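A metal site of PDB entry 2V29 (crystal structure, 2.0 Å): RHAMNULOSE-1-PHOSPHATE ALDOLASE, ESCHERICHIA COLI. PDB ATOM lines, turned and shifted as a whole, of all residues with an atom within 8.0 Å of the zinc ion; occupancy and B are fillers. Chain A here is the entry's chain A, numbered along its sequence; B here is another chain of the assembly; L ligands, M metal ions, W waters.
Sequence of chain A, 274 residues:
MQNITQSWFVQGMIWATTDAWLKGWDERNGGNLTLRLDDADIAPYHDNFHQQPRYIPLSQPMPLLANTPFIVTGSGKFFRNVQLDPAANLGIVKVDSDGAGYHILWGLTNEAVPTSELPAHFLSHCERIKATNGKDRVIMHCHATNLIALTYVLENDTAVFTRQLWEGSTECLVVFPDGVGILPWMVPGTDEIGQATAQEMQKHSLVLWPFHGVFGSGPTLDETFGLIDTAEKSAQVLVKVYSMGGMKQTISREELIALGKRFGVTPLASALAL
The backbone carbonyl oxygen (O) of Trp 25 sits at hydrogen-bond distance from the backbone NH (N) of His 143 (2.8 Å).
The backbone NH (N) of His 141 lies within hydrogen-bond range of the backbone carbonyl oxygen (O) of Asn 32, at 2.8 Å.
ND1 of His 143 lies within hydrogen-bond range of OE1 of Glu 27 (2.8 Å).
ND1 of His 141 lies within hydrogen-bond range of O of Val 214 (2.9 Å).
Within 4 Å of the zinc ion: His 141, His 143 and His 212.
Along chain A the residues within 4 Å of the zinc ion span positions 141 to 212.
The nearest printed residue that does not touch the zinc ion is Gly 31 (4.4 Å).
The zinc ion is bound by O2 of the ligand, 2.0 Å away.
The zinc ion is bound by NE2 of His 212 (2.1 Å).
A ring nitrogen (NE2) of His 141 binds the zinc ion (2.1 Å).
The zinc ion is bound by NE2 of His 143, 2.1 Å away.
O1 of the ligand is bound to the zinc ion.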
ATOM      1  N   TRP A  25      -7.783   5.880  -8.145  1.00  0.00           N
ATOM      2  CA  TRP A  25      -7.733   4.995  -9.311  1.00  0.00           C
ATOM      3  C   TRP A  25      -8.642   3.780  -9.207  1.00  0.00           C
ATOM      4  O   TRP A  25      -8.696   2.974 -10.128  1.00  0.00           O
ATOM      5  CB  TRP A  25      -6.316   4.441  -9.521  1.00  0.00           C
ATOM      6  CG  TRP A  25      -5.240   5.482  -9.727  1.00  0.00           C
ATOM      7  CD1 TRP A  25      -5.393   6.801 -10.039  1.00  0.00           C
ATOM      8  CD2 TRP A  25      -3.831   5.239  -9.668  1.00  0.00           C
ATOM      9  NE1 TRP A  25      -4.152   7.409 -10.164  1.00  0.00           N
ATOM     10  CE2 TRP A  25      -3.180   6.464  -9.928  1.00  0.00           C
ATOM     11  CE3 TRP A  25      -3.060   4.099  -9.378  1.00  0.00           C
ATOM     12  CZ2 TRP A  25      -1.795   6.580  -9.931  1.00  0.00           C
ATOM     13  CZ3 TRP A  25      -1.665   4.213  -9.384  1.00  0.00           C
ATOM     14  CH2 TRP A  25      -1.049   5.432  -9.674  1.00  0.00           C
ATOM     15  N   ASP A  26      -9.300   3.598  -8.066  1.00  0.00           N
ATOM     16  CA  ASP A  26      -9.958   2.305  -7.831  1.00  0.00           C
ATOM     17  C   ASP A  26     -11.282   2.422  -7.044  1.00  0.00           C
ATOM     18  O   ASP A  26     -11.468   1.807  -5.976  1.00  0.00           O
ATOM     19  CB  ASP A  26      -8.978   1.337  -7.188  1.00  0.00           C
ATOM     20  CG  ASP A  26      -7.831   0.968  -8.133  1.00  0.00           C
ATOM     21  OD1 ASP A  26      -6.702   1.519  -7.995  1.00  0.00           O
ATOM     22  OD2 ASP A  26      -8.059   0.152  -9.066  1.00  0.00           O
ATOM     23  N   GLU A  27     -12.210   3.188  -7.636  1.00  0.00           N
ATOM     24  CA  GLU A  27     -13.614   3.312  -7.202  1.00  0.00           C
ATOM     25  C   GLU A  27     -14.244   1.915  -7.160  1.00  0.00           C
ATOM     26  O   GLU A  27     -13.908   1.052  -7.982  1.00  0.00           O
ATOM     27  CB  GLU A  27     -14.411   4.217  -8.180  1.00  0.00           C
ATOM     28  CG  GLU A  27     -14.615   3.647  -9.625  1.00  0.00           C
ATOM     29  CD  GLU A  27     -13.418   3.830 -10.552  1.00  0.00           C
ATOM     30  OE1 GLU A  27     -13.541   3.462 -11.737  1.00  0.00           O
ATOM     31  OE2 GLU A  27     -12.337   4.355 -10.124  1.00  0.00           O
ATOM     32  N   ASN A  29     -15.188  -1.699  -7.133  1.00  0.00           N
ATOM     33  CA  ASN A  29     -14.313  -2.852  -7.390  1.00  0.00           C
ATOM     34  C   ASN A  29     -13.379  -2.658  -8.601  1.00  0.00           C
ATOM     35  O   ASN A  29     -12.828  -3.648  -9.123  1.00  0.00           O
ATOM     36  CB  ASN A  29     -15.165  -4.126  -7.579  1.00  0.00           C
ATOM     37  CG  ASN A  29     -16.046  -4.042  -8.812  1.00  0.00           C
ATOM     38  OD1 ASN A  29     -16.751  -3.054  -8.992  1.00  0.00           O
ATOM     39  ND2 ASN A  29     -16.002  -5.066  -9.667  1.00  0.00           N
ATOM     40  N   GLY A  30     -13.246  -1.412  -9.067  1.00  0.00           N
ATOM     41  CA  GLY A  30     -12.451  -1.087 -10.242  1.00  0.00           C
ATOM     42  C   GLY A  30     -11.020  -1.459  -9.921  1.00  0.00           C
ATOM     43  O   GLY A  30     -10.491  -1.052  -8.891  1.00  0.00           O
ATOM     44  N   GLY A  31     -10.403  -2.290 -10.756  1.00  0.00           N
ATOM     45  CA  GLY A  31      -8.982  -2.601 -10.562  1.00  0.00           C
ATOM     46  C   GLY A  31      -8.744  -4.013 -10.053  1.00  0.00           C
ATOM     47  O   GLY A  31      -9.599  -4.626  -9.389  1.00  0.00           O
ATOM     48  N   ASN A  32      -7.570  -4.558 -10.377  1.00  0.00           N
ATOM     49  CA  ASN A  32      -7.177  -5.866  -9.859  1.00  0.00           C
ATOM     50  C   ASN A  32      -5.668  -6.034  -9.910  1.00  0.00           C
ATOM     51  O   ASN A  32      -4.956  -5.345 -10.650  1.00  0.00           O
ATOM     52  CB  ASN A  32      -7.931  -6.989 -10.583  1.00  0.00           C
ATOM     53  CG  ASN A  32      -8.365  -6.600 -11.995  1.00  0.00           C
ATOM     54  OD1 ASN A  32      -7.550  -6.515 -12.923  1.00  0.00           O
ATOM     55  ND2 ASN A  32      -9.647  -6.357 -12.155  1.00  0.00           N
ATOM     56  N   GLU A 117     -10.972 -11.538 -13.821  1.00  0.00           N
ATOM     57  CA  GLU A 117      -9.898 -11.356 -14.779  1.00  0.00           C
ATOM     58  C   GLU A 117      -8.638 -12.152 -14.480  1.00  0.00           C
ATOM     59  O   GLU A 117      -7.584 -11.845 -15.012  1.00  0.00           O
ATOM     60  CB  GLU A 117      -9.563  -9.871 -14.901  1.00  0.00           C
ATOM     61  CG  GLU A 117     -10.760  -9.088 -15.339  1.00  0.00           C
ATOM     62  CD  GLU A 117     -10.420  -7.932 -16.232  1.00  0.00           C
ATOM     63  OE1 GLU A 117     -10.829  -7.966 -17.420  1.00  0.00           O
ATOM     64  OE2 GLU A 117      -9.752  -6.986 -15.740  1.00  0.00           O
ATOM     65  N   HIS A 141      -3.895  -3.753 -12.732  1.00  0.00           N
ATOM     66  CA  HIS A 141      -4.899  -3.001 -13.479  1.00  0.00           C
ATOM     67  C   HIS A 141      -5.516  -1.935 -12.558  1.00  0.00           C
ATOM     68  O   HIS A 141      -5.843  -2.228 -11.428  1.00  0.00           O
ATOM     69  CB  HIS A 141      -5.972  -3.942 -14.072  1.00  0.00           C
ATOM     70  CG  HIS A 141      -7.194  -3.234 -14.581  1.00  0.00           C
ATOM     71  ND1 HIS A 141      -7.141  -2.280 -15.580  1.00  0.00           N
ATOM     72  CD2 HIS A 141      -8.500  -3.353 -14.260  1.00  0.00           C
ATOM     73  CE1 HIS A 141      -8.354  -1.827 -15.825  1.00  0.00           C
ATOM     74  NE2 HIS A 141      -9.204  -2.474 -15.040  1.00  0.00           N
ATOM     75  N   CYS A 142      -5.627  -0.699 -13.043  1.00  0.00           N
ATOM     76  CA  CYS A 142      -6.376   0.306 -12.302  1.00  0.00           C
ATOM     77  C   CYS A 142      -7.006   1.322 -13.246  1.00  0.00           C
ATOM     78  O   CYS A 142      -6.691   1.356 -14.448  1.00  0.00           O
ATOM     79  CB  CYS A 142      -5.497   1.038 -11.289  1.00  0.00           C
ATOM     80  SG  CYS A 142      -4.217   1.932 -12.058  1.00  0.00           S
ATOM     81  N   HIS A 143      -7.896   2.116 -12.684  1.00  0.00           N
ATOM     82  CA  HIS A 143      -8.635   3.089 -13.450  1.00  0.00           C
ATOM     83  C   HIS A 143      -7.998   4.460 -13.285  1.00  0.00           C
ATOM     84  O   HIS A 143      -8.547   5.357 -12.664  1.00  0.00           O
ATOM     85  CB  HIS A 143     -10.102   3.047 -13.059  1.00  0.00           C
ATOM     86  CG  HIS A 143     -10.769   1.750 -13.409  1.00  0.00           C
ATOM     87  ND1 HIS A 143     -12.051   1.456 -13.016  1.00  0.00           N
ATOM     88  CD2 HIS A 143     -10.292   0.654 -14.044  1.00  0.00           C
ATOM     89  CE1 HIS A 143     -12.364   0.243 -13.461  1.00  0.00           C
ATOM     90  NE2 HIS A 143     -11.305  -0.274 -14.071  1.00  0.00           N
ATOM     91  N   ILE A 148      -7.204   7.674 -18.480  1.00  0.00           N
ATOM     92  CA  ILE A 148      -8.563   7.491 -19.013  1.00  0.00           C
ATOM     93  C   ILE A 148      -9.049   8.744 -19.787  1.00  0.00           C
ATOM     94  O   ILE A 148      -9.463   8.653 -20.947  1.00  0.00           O
ATOM     95  CB  ILE A 148      -9.576   7.134 -17.887  1.00  0.00           C
ATOM     96  CG1 ILE A 148      -9.248   5.758 -17.286  1.00  0.00           C
ATOM     97  CG2 ILE A 148     -11.055   7.129 -18.456  1.00  0.00           C
ATOM     98  CD1 ILE A 148      -9.931   5.482 -15.887  1.00  0.00           C
ATOM     99  N   PRO A 188     -14.950  -5.763 -21.491  1.00  0.00           N
ATOM    100  CA  PRO A 188     -14.040  -6.289 -20.466  1.00  0.00           C
ATOM    101  C   PRO A 188     -14.422  -7.690 -19.958  1.00  0.00           C
ATOM    102  O   PRO A 188     -15.581  -8.122 -20.116  1.00  0.00           O
ATOM    103  CB  PRO A 188     -14.173  -5.289 -19.310  1.00  0.00           C
ATOM    104  CG  PRO A 188     -15.086  -4.225 -19.762  1.00  0.00           C
ATOM    105  CD  PRO A 188     -15.805  -4.684 -20.987  1.00  0.00           C
ATOM    106  N   GLY A 189     -13.470  -8.373 -19.336  1.00  0.00           N
ATOM    107  CA  GLY A 189     -13.693  -9.713 -18.808  1.00  0.00           C
ATOM    108  C   GLY A 189     -13.845 -10.809 -19.857  1.00  0.00           C
ATOM    109  O   GLY A 189     -14.163 -11.950 -19.487  1.00  0.00           O
ATOM    110  N   TRP A 209      -6.525   0.539 -22.161  1.00  0.00           N
ATOM    111  CA  TRP A 209      -7.859   0.142 -22.563  1.00  0.00           C
ATOM    112  C   TRP A 209      -8.652   1.437 -22.620  1.00  0.00           C
ATOM    113  O   TRP A 209      -9.015   1.959 -21.597  1.00  0.00           O
ATOM    114  CB  TRP A 209      -8.445  -0.740 -21.446  1.00  0.00           C
ATOM    115  CG  TRP A 209      -7.904  -2.145 -21.414  1.00  0.00           C
ATOM    116  CD1 TRP A 209      -6.897  -2.674 -22.206  1.00  0.00           C
ATOM    117  CD2 TRP A 209      -8.326  -3.168 -20.544  1.00  0.00           C
ATOM    118  NE1 TRP A 209      -6.672  -3.983 -21.859  1.00  0.00           N
ATOM    119  CE2 TRP A 209      -7.530  -4.316 -20.838  1.00  0.00           C
ATOM    120  CE3 TRP A 209      -9.299  -3.250 -19.542  1.00  0.00           C
ATOM    121  CZ2 TRP A 209      -7.714  -5.545 -20.175  1.00  0.00           C
ATOM    122  CZ3 TRP A 209      -9.488  -4.451 -18.885  1.00  0.00           C
ATOM    123  CH2 TRP A 209      -8.695  -5.608 -19.207  1.00  0.00           C
ATOM    124  N   PHE A 211     -11.181   4.464 -22.596  1.00  0.00           N
ATOM    125  CA  PHE A 211     -12.432   4.662 -21.851  1.00  0.00           C
ATOM    126  C   PHE A 211     -12.564   3.752 -20.633  1.00  0.00           C
ATOM    127  O   PHE A 211     -13.676   3.524 -20.138  1.00  0.00           O
ATOM    128  CB  PHE A 211     -13.681   4.481 -22.784  1.00  0.00           C
ATOM    129  CG  PHE A 211     -13.469   4.972 -24.209  1.00  0.00           C
ATOM    130  CD1 PHE A 211     -13.874   4.178 -25.298  1.00  0.00           C
ATOM    131  CD2 PHE A 211     -12.854   6.207 -24.455  1.00  0.00           C
ATOM    132  CE1 PHE A 211     -13.651   4.620 -26.601  1.00  0.00           C
ATOM    133  CE2 PHE A 211     -12.637   6.647 -25.745  1.00  0.00           C
ATOM    134  CZ  PHE A 211     -13.047   5.844 -26.839  1.00  0.00           C
ATOM    135  N   HIS A 212     -11.456   3.179 -20.174  1.00  0.00           N
ATOM    136  CA  HIS A 212     -11.538   2.199 -19.089  1.00  0.00           C
ATOM    137  C   HIS A 212     -10.358   2.309 -18.111  1.00  0.00           C
ATOM    138  O   HIS A 212     -10.534   2.618 -16.912  1.00  0.00           O
ATOM    139  CB  HIS A 212     -11.625   0.789 -19.722  1.00  0.00           C
ATOM    140  CG  HIS A 212     -11.761  -0.324 -18.735  1.00  0.00           C
ATOM    141  ND1 HIS A 212     -12.228  -1.581 -19.086  1.00  0.00           N
ATOM    142  CD2 HIS A 212     -11.472  -0.391 -17.412  1.00  0.00           C
ATOM    143  CE1 HIS A 212     -12.234  -2.349 -18.018  1.00  0.00           C
ATOM    144  NE2 HIS A 212     -11.767  -1.671 -16.997  1.00  0.00           N
ATOM    145  N   GLY A 213      -9.139   2.029 -18.566  1.00  0.00           N
ATOM    146  CA  GLY A 213      -8.009   2.063 -17.606  1.00  0.00           C
ATOM    147  C   GLY A 213      -6.701   1.527 -18.191  1.00  0.00           C
ATOM    148  O   GLY A 213      -6.523   1.471 -19.424  1.00  0.00           O
ATOM    149  N   VAL A 214      -5.793   1.182 -17.298  1.00  0.00           N
ATOM    150  CA  VAL A 214      -4.417   0.827 -17.669  1.00  0.00           C
ATOM    151  C   VAL A 214      -4.066  -0.531 -17.051  1.00  0.00           C
ATOM    152  O   VAL A 214      -4.653  -0.931 -16.026  1.00  0.00           O
ATOM    153  CB  VAL A 214      -3.393   1.935 -17.263  1.00  0.00           C
ATOM    154  CG1 VAL A 214      -3.304   2.091 -15.732  1.00  0.00           C
ATOM    155  CG2 VAL A 214      -1.989   1.702 -17.876  1.00  0.00           C
ATOM    156  N   PHE A 215      -3.134  -1.211 -17.699  1.00  0.00           N
ATOM    157  CA  PHE A 215      -2.521  -2.470 -17.275  1.00  0.00           C
ATOM    158  C   PHE A 215      -1.015  -2.359 -17.308  1.00  0.00           C
ATOM    159  O   PHE A 215      -0.441  -1.965 -18.334  1.00  0.00           O
ATOM    160  CB  PHE A 215      -2.882  -3.568 -18.264  1.00  0.00           C
ATOM    161  CG  PHE A 215      -4.007  -4.397 -17.823  1.00  0.00           C
ATOM    162  CD1 PHE A 215      -5.300  -3.927 -17.946  1.00  0.00           C
ATOM    163  CD2 PHE A 215      -3.789  -5.616 -17.247  1.00  0.00           C
ATOM    164  CE1 PHE A 215      -6.348  -4.702 -17.491  1.00  0.00           C
ATOM    165  CE2 PHE A 215      -4.819  -6.395 -16.800  1.00  0.00           C
ATOM    166  CZ  PHE A 215      -6.108  -5.935 -16.906  1.00  0.00           C
ATOM    167  N   THR B 170     -16.110   2.836 -18.607  1.00  0.00           N
ATOM    168  CA  THR B 170     -16.740   1.622 -19.177  1.00  0.00           C
ATOM    169  C   THR B 170     -17.702   0.906 -18.206  1.00  0.00           C
ATOM    170  O   THR B 170     -18.791   0.501 -18.599  1.00  0.00           O
ATOM    171  CB  THR B 170     -15.658   0.664 -19.782  1.00  0.00           C
ATOM    172  OG1 THR B 170     -15.094   1.307 -20.900  1.00  0.00           O
ATOM    173  CG2 THR B 170     -16.280  -0.688 -20.291  1.00  0.00           C
ATOM    174  N   GLU B 171     -17.312   0.824 -16.926  1.00  0.00           N
ATOM    175  CA  GLU B 171     -18.123   0.150 -15.909  1.00  0.00           C
ATOM    176  C   GLU B 171     -19.480   0.788 -15.606  1.00  0.00           C
ATOM    177  O   GLU B 171     -20.325   0.108 -15.041  1.00  0.00           O
ATOM    178  CB  GLU B 171     -17.359   0.096 -14.573  1.00  0.00           C
ATOM    179  CG  GLU B 171     -17.288   1.492 -13.945  1.00  0.00           C
ATOM    180  CD  GLU B 171     -16.142   1.726 -12.970  1.00  0.00           C
ATOM    181  OE1 GLU B 171     -15.518   0.763 -12.475  1.00  0.00           O
ATOM    182  OE2 GLU B 171     -15.880   2.909 -12.694  1.00  0.00           O
HETATM  183  C1  LIG L   1     -12.541  -3.639 -13.436  1.00  0.00           C
HETATM  184  O1  LIG L   1     -11.415  -3.382 -13.041  1.00  0.00           O
HETATM  185  O2  LIG L   1     -12.969  -3.045 -14.442  1.00  0.00           O
HETATM  186  C2  LIG L   1     -13.390  -4.658 -12.722  1.00  0.00           C
HETATM  187 ZN    ZN M   1     -11.270  -2.138 -15.057  1.00  0.00          ZN
HETATM  188  O   HOH W   1     -11.711  -4.943 -15.852  1.00  0.00           O
